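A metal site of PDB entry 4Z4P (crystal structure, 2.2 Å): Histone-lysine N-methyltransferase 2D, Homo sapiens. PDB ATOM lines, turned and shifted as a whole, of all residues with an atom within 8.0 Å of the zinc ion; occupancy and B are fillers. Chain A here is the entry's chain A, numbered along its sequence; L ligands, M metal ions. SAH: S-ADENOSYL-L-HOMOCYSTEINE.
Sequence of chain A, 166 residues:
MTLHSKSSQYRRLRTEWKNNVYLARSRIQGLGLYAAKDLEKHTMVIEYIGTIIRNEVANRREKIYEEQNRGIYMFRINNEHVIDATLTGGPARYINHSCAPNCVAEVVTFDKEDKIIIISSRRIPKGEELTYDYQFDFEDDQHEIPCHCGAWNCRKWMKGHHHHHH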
ATOM      1  N   ILE A  28      23.907 -30.942 -31.262  1.00  0.00           N
ATOM      2  CA  ILE A  28      23.829 -30.453 -29.897  1.00  0.00           C
ATOM      3  C   ILE A  28      23.280 -31.526 -28.961  1.00  0.00           C
ATOM      4  O   ILE A  28      23.973 -31.962 -28.050  1.00  0.00           O
ATOM      5  CB  ILE A  28      22.976 -29.184 -29.816  1.00  0.00           C
ATOM      6  CG1 ILE A  28      23.695 -28.060 -30.576  1.00  0.00           C
ATOM      7  CG2 ILE A  28      22.729 -28.766 -28.394  1.00  0.00           C
ATOM      8  CD1 ILE A  28      22.867 -26.818 -30.763  1.00  0.00           C
ATOM      9  N   HIS A  97      18.191 -25.423 -28.036  1.00  0.00           N
ATOM     10  CA  HIS A  97      18.743 -24.226 -27.436  1.00  0.00           C
ATOM     11  C   HIS A  97      20.229 -24.014 -27.745  1.00  0.00           C
ATOM     12  O   HIS A  97      21.018 -24.966 -27.747  1.00  0.00           O
ATOM     13  CB  HIS A  97      18.575 -24.272 -25.904  1.00  0.00           C
ATOM     14  CG  HIS A  97      19.406 -23.256 -25.178  1.00  0.00           C
ATOM     15  ND1 HIS A  97      19.056 -21.929 -25.101  1.00  0.00           N
ATOM     16  CD2 HIS A  97      20.602 -23.379 -24.560  1.00  0.00           C
ATOM     17  CE1 HIS A  97      19.987 -21.271 -24.430  1.00  0.00           C
ATOM     18  NE2 HIS A  97      20.935 -22.121 -24.092  1.00  0.00           N
ATOM     19  N   SER A  98      20.618 -22.770 -27.983  1.00  0.00           N
ATOM     20  CA  SER A  98      22.043 -22.432 -27.978  1.00  0.00           C
ATOM     21  C   SER A  98      22.263 -21.100 -27.278  1.00  0.00           C
ATOM     22  O   SER A  98      21.489 -20.140 -27.435  1.00  0.00           O
ATOM     23  CB  SER A  98      22.619 -22.382 -29.390  1.00  0.00           C
ATOM     24  OG  SER A  98      23.943 -21.860 -29.381  1.00  0.00           O
ATOM     25  N   CYS A  99      23.337 -21.039 -26.505  1.00  0.00           N
ATOM     26  CA  CYS A  99      23.758 -19.808 -25.850  1.00  0.00           C
ATOM     27  C   CYS A  99      24.295 -18.819 -26.890  1.00  0.00           C
ATOM     28  O   CYS A  99      24.456 -17.639 -26.609  1.00  0.00           O
ATOM     29  CB  CYS A  99      24.804 -20.119 -24.786  1.00  0.00           C
ATOM     30  SG  CYS A  99      24.136 -21.096 -23.418  1.00  0.00           S
ATOM     31  N   ALA A 100      24.580 -19.328 -28.091  1.00  0.00           N
ATOM     32  CA  ALA A 100      24.932 -18.495 -29.248  1.00  0.00           C
ATOM     33  C   ALA A 100      24.106 -18.919 -30.452  1.00  0.00           C
ATOM     34  O   ALA A 100      24.595 -19.639 -31.325  1.00  0.00           O
ATOM     35  CB  ALA A 100      26.409 -18.611 -29.554  1.00  0.00           C
ATOM     36  N   PRO A 146      22.095 -29.440 -17.407  1.00  0.00           N
ATOM     37  CA  PRO A 146      23.306 -29.020 -18.103  1.00  0.00           C
ATOM     38  C   PRO A 146      23.070 -28.619 -19.562  1.00  0.00           C
ATOM     39  O   PRO A 146      22.309 -29.282 -20.281  1.00  0.00           O
ATOM     40  CB  PRO A 146      24.203 -30.264 -18.048  1.00  0.00           C
ATOM     41  CG  PRO A 146      23.740 -31.022 -16.836  1.00  0.00           C
ATOM     42  CD  PRO A 146      22.276 -30.728 -16.692  1.00  0.00           C
ATOM     43  N   CYS A 147      23.712 -27.533 -19.979  1.00  0.00           N
ATOM     44  CA  CYS A 147      23.667 -27.128 -21.368  1.00  0.00           C
ATOM     45  C   CYS A 147      24.876 -27.693 -22.094  1.00  0.00           C
ATOM     46  O   CYS A 147      26.008 -27.644 -21.589  1.00  0.00           O
ATOM     47  CB  CYS A 147      23.636 -25.599 -21.497  1.00  0.00           C
ATOM     48  SG  CYS A 147      23.559 -25.007 -23.207  1.00  0.00           S
ATOM     49  N   HIS A 148      24.633 -28.256 -23.270  1.00  0.00           N
ATOM     50  CA  HIS A 148      25.678 -28.891 -24.046  1.00  0.00           C
ATOM     51  C   HIS A 148      25.719 -28.275 -25.433  1.00  0.00           C
ATOM     52  O   HIS A 148      26.051 -28.950 -26.399  1.00  0.00           O
ATOM     53  CB  HIS A 148      25.451 -30.411 -24.150  1.00  0.00           C
ATOM     54  CG  HIS A 148      25.589 -31.132 -22.849  1.00  0.00           C
ATOM     55  ND1 HIS A 148      26.721 -31.032 -22.063  1.00  0.00           N
ATOM     56  CD2 HIS A 148      24.751 -31.970 -22.205  1.00  0.00           C
ATOM     57  CE1 HIS A 148      26.558 -31.773 -20.977  1.00  0.00           C
ATOM     58  NE2 HIS A 148      25.374 -32.350 -21.035  1.00  0.00           N
ATOM     59  N   CYS A 149      25.391 -26.990 -25.519  1.00  0.00           N
ATOM     60  CA  CYS A 149      25.314 -26.316 -26.818  1.00  0.00           C
ATOM     61  C   CYS A 149      26.704 -26.142 -27.426  1.00  0.00           C
ATOM     62  O   CYS A 149      26.849 -26.013 -28.644  1.00  0.00           O
ATOM     63  CB  CYS A 149      24.625 -24.947 -26.693  1.00  0.00           C
ATOM     64  SG  CYS A 149      25.585 -23.545 -25.982  1.00  0.00           S
ATOM     65  N   GLY A 150      27.709 -26.140 -26.551  1.00  0.00           N
ATOM     66  CA  GLY A 150      29.106 -26.115 -26.976  1.00  0.00           C
ATOM     67  C   GLY A 150      29.649 -24.771 -27.422  1.00  0.00           C
ATOM     68  O   GLY A 150      30.764 -24.712 -27.948  1.00  0.00           O
ATOM     69  N   ALA A 151      28.898 -23.697 -27.229  1.00  0.00           N
ATOM     70  CA  ALA A 151      29.361 -22.381 -27.655  1.00  0.00           C
ATOM     71  C   ALA A 151      30.319 -21.793 -26.634  1.00  0.00           C
ATOM     72  O   ALA A 151      30.352 -22.218 -25.472  1.00  0.00           O
ATOM     73  CB  ALA A 151      28.192 -21.435 -27.876  1.00  0.00           C
ATOM     74  N   TRP A 152      31.105 -20.810 -27.079  1.00  0.00           N
ATOM     75  CA  TRP A 152      32.142 -20.196 -26.268  1.00  0.00           C
ATOM     76  C   TRP A 152      31.602 -19.558 -24.993  1.00  0.00           C
ATOM     77  O   TRP A 152      32.236 -19.637 -23.943  1.00  0.00           O
ATOM     78  CB  TRP A 152      32.890 -19.141 -27.086  1.00  0.00           C
ATOM     79  CG  TRP A 152      31.982 -18.032 -27.526  1.00  0.00           C
ATOM     80  CD1 TRP A 152      31.138 -18.037 -28.606  1.00  0.00           C
ATOM     81  CD2 TRP A 152      31.816 -16.754 -26.898  1.00  0.00           C
ATOM     82  NE1 TRP A 152      30.461 -16.843 -28.688  1.00  0.00           N
ATOM     83  CE2 TRP A 152      30.860 -16.040 -27.646  1.00  0.00           C
ATOM     84  CE3 TRP A 152      32.389 -16.139 -25.768  1.00  0.00           C
ATOM     85  CZ2 TRP A 152      30.455 -14.738 -27.302  1.00  0.00           C
ATOM     86  CZ3 TRP A 152      31.980 -14.842 -25.437  1.00  0.00           C
ATOM     87  CH2 TRP A 152      31.026 -14.161 -26.203  1.00  0.00           C
ATOM     88  N   ASN A 153      30.430 -18.935 -25.087  1.00  0.00           N
ATOM     89  CA  ASN A 153      29.874 -18.227 -23.950  1.00  0.00           C
ATOM     90  C   ASN A 153      28.792 -19.021 -23.238  1.00  0.00           C
ATOM     91  O   ASN A 153      27.989 -18.450 -22.504  1.00  0.00           O
ATOM     92  CB  ASN A 153      29.312 -16.868 -24.377  1.00  0.00           C
ATOM     93  CG  ASN A 153      28.081 -17.001 -25.248  1.00  0.00           C
ATOM     94  OD1 ASN A 153      27.974 -17.935 -26.037  1.00  0.00           O
ATOM     95  ND2 ASN A 153      27.154 -16.068 -25.095  1.00  0.00           N
ATOM     96  N   CYS A 154      28.768 -20.325 -23.456  1.00  0.00           N
ATOM     97  CA  CYS A 154      27.738 -21.185 -22.898  1.00  0.00           C
ATOM     98  C   CYS A 154      27.624 -21.015 -21.389  1.00  0.00           C
ATOM     99  O   CYS A 154      28.599 -21.136 -20.659  1.00  0.00           O
ATOM    100  CB  CYS A 154      28.012 -22.647 -23.253  1.00  0.00           C
ATOM    101  SG  CYS A 154      26.939 -23.853 -22.402  1.00  0.00           S
ATOM    102  N   ARG A 155      26.400 -20.725 -20.945  1.00  0.00           N
ATOM    103  CA  ARG A 155      26.105 -20.526 -19.548  1.00  0.00           C
ATOM    104  C   ARG A 155      25.987 -21.858 -18.799  1.00  0.00           C
ATOM    105  O   ARG A 155      25.597 -21.903 -17.635  1.00  0.00           O
ATOM    106  CB  ARG A 155      24.816 -19.718 -19.417  1.00  0.00           C
ATOM    107  CG  ARG A 155      24.504 -18.903 -20.677  1.00  0.00           C
ATOM    108  CD  ARG A 155      23.502 -17.781 -20.409  1.00  0.00           C
ATOM    109  NE  ARG A 155      23.983 -16.880 -19.363  1.00  0.00           N
ATOM    110  CZ  ARG A 155      23.234 -15.981 -18.725  1.00  0.00           C
ATOM    111  NH1 ARG A 155      23.772 -15.207 -17.792  1.00  0.00           N
ATOM    112  NH2 ARG A 155      21.948 -15.858 -19.022  1.00  0.00           N
ATOM    113  N   LYS A 156      26.314 -22.959 -19.504  1.00  0.00           N
ATOM    114  CA  LYS A 156      26.482 -24.298 -18.915  1.00  0.00           C
ATOM    115  C   LYS A 156      25.239 -24.889 -18.278  1.00  0.00           C
ATOM    116  O   LYS A 156      25.241 -26.041 -17.867  1.00  0.00           O
ATOM    117  CB  LYS A 156      27.623 -24.289 -17.900  1.00  0.00           C
ATOM    118  CG  LYS A 156      28.993 -24.217 -18.537  1.00  0.00           C
ATOM    119  CD  LYS A 156      29.313 -25.519 -19.279  1.00  0.00           C
ATOM    120  CE  LYS A 156      30.533 -25.356 -20.186  1.00  0.00           C
ATOM    121  NZ  LYS A 156      31.712 -24.796 -19.464  1.00  0.00           N
ATOM    122  N   TRP A 157      24.179 -24.087 -18.195  1.00  0.00           N
ATOM    123  CA  TRP A 157      22.902 -24.576 -17.689  1.00  0.00           C
ATOM    124  C   TRP A 157      21.785 -24.013 -18.556  1.00  0.00           C
ATOM    125  O   TRP A 157      21.968 -23.001 -19.231  1.00  0.00           O
ATOM    126  CB  TRP A 157      22.709 -24.179 -16.217  1.00  0.00           C
ATOM    127  CG  TRP A 157      23.712 -24.833 -15.285  1.00  0.00           C
ATOM    128  CD1 TRP A 157      24.927 -24.348 -14.900  1.00  0.00           C
ATOM    129  CD2 TRP A 157      23.571 -26.109 -14.642  1.00  0.00           C
ATOM    130  NE1 TRP A 157      25.547 -25.236 -14.057  1.00  0.00           N
ATOM    131  CE2 TRP A 157      24.738 -26.328 -13.885  1.00  0.00           C
ATOM    132  CE3 TRP A 157      22.568 -27.092 -14.629  1.00  0.00           C
ATOM    133  CZ2 TRP A 157      24.936 -27.483 -13.122  1.00  0.00           C
ATOM    134  CZ3 TRP A 157      22.769 -28.238 -13.871  1.00  0.00           C
ATOM    135  CH2 TRP A 157      23.938 -28.416 -13.124  1.00  0.00           C
ATOM    136  N   MET A 158      20.643 -24.677 -18.516  1.00  0.00           N
ATOM    137  CA  MET A 158      19.470 -24.271 -19.289  1.00  0.00           C
ATOM    138  C   MET A 158      18.245 -24.853 -18.605  1.00  0.00           C
ATOM    139  O   MET A 158      18.382 -25.688 -17.709  1.00  0.00           O
ATOM    140  CB  MET A 158      19.549 -24.778 -20.712  1.00  0.00           C
ATOM    141  CG  MET A 158      19.373 -26.287 -20.747  1.00  0.00           C
ATOM    142  SD  MET A 158      19.291 -26.991 -22.380  1.00  0.00           S
ATOM    143  CE  MET A 158      17.674 -26.472 -22.922  1.00  0.00           C
HETATM  144  N   SAH L   1      16.650 -32.310 -28.784  1.00  0.00           N
HETATM  145  CA  SAH L   1      15.256 -32.450 -28.405  1.00  0.00           C
HETATM  146  CB  SAH L   1      14.436 -31.338 -29.049  1.00  0.00           C
HETATM  147  CG  SAH L   1      14.673 -30.004 -28.338  1.00  0.00           C
HETATM  148  SD  SAH L   1      13.335 -29.696 -27.230  1.00  0.00           S
HETATM  149  C   SAH L   1      14.733 -33.775 -28.861  1.00  0.00           C
HETATM  150  O   SAH L   1      15.497 -34.509 -29.527  1.00  0.00           O
HETATM  151  OXT SAH L   1      13.563 -34.102 -28.553  1.00  0.00           O
HETATM  152  C5' SAH L   1      14.250 -29.220 -25.795  1.00  0.00           C
HETATM  153  C4' SAH L   1      14.911 -30.449 -25.181  1.00  0.00           C
HETATM  154  O4' SAH L   1      16.135 -30.729 -25.877  1.00  0.00           O
HETATM  155  C3' SAH L   1      15.246 -30.222 -23.724  1.00  0.00           C
HETATM  156  O3' SAH L   1      14.575 -31.192 -22.909  1.00  0.00           O
HETATM  157  C2' SAH L   1      16.747 -30.388 -23.599  1.00  0.00           C
HETATM  158  O2' SAH L   1      17.049 -31.467 -22.708  1.00  0.00           O
HETATM  159  C1' SAH L   1      17.261 -30.703 -24.992  1.00  0.00           C
HETATM  160  N9  SAH L   1      18.223 -29.662 -25.427  1.00  0.00           N
HETATM  161  C8  SAH L   1      17.994 -28.732 -26.377  1.00  0.00           C
HETATM  162  N7  SAH L   1      19.074 -27.918 -26.530  1.00  0.00           N
HETATM  163  C5  SAH L   1      20.019 -28.333 -25.670  1.00  0.00           C
HETATM  164  C6  SAH L   1      21.400 -27.923 -25.316  1.00  0.00           C
HETATM  165  N6  SAH L   1      21.990 -26.880 -25.932  1.00  0.00           N
HETATM  166  N1  SAH L   1      22.035 -28.627 -24.351  1.00  0.00           N
HETATM  167  C2  SAH L   1      21.453 -29.669 -23.731  1.00  0.00           C
HETATM  168  N3  SAH L   1      20.207 -30.098 -23.996  1.00  0.00           N
HETATM  169  C4  SAH L   1      19.451 -29.484 -24.942  1.00  0.00           C
HETATM  170 ZN    ZN M   1      25.029 -23.426 -23.819  1.00  0.00          ZN
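Within 4 Å of the zinc ion: Cys 99, Cys 147, Cys 149 and Cys 154.
N6 of the ligand lies close to SG of Cys 147 (3.7 Å). The backbone NH (N) of His 97 lies within hydrogen-bond range of a nitrogen (N7) of the ligand, at 3.0 Å. The backbone carbonyl oxygen (O) of His 97 is in hydrogen-bond range of a nitrogen (N6) of the ligand (2.8 Å). The backbone NH (N) of His 148 sits at hydrogen-bond distance from a nitrogen (N1) of the ligand, at 2.8 Å.
The side-chain sulfur (SG) of Cys 149 sits close to the backbone NH (N) of Ala 151 (3.5 Å). N of Cys 147 is in hydrogen-bond range of O of Lys 156, 3.0 Å away. The side-chain sulfur of Cys 154 sits close to the backbone NH of Lys 156. SG of Cys 99 sits close to N of Arg 155. The side-chain sulfur of Cys 99 sits close to a ring nitrogen (NE2) of His 97, 3.4 Å away. ND2 of Asn 153 is in hydrogen-bond range of O of Cys 99 (3.5 Å).
The zinc ion is bound by SG of Cys 149. SG of Cys 147 binds the zinc ion (2.2 Å). The zinc ion is bound by the side-chain sulfur (SG) of Cys 154 (2.4 Å). The zinc ion is bound by SG of Cys 99 (2.5 Å).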
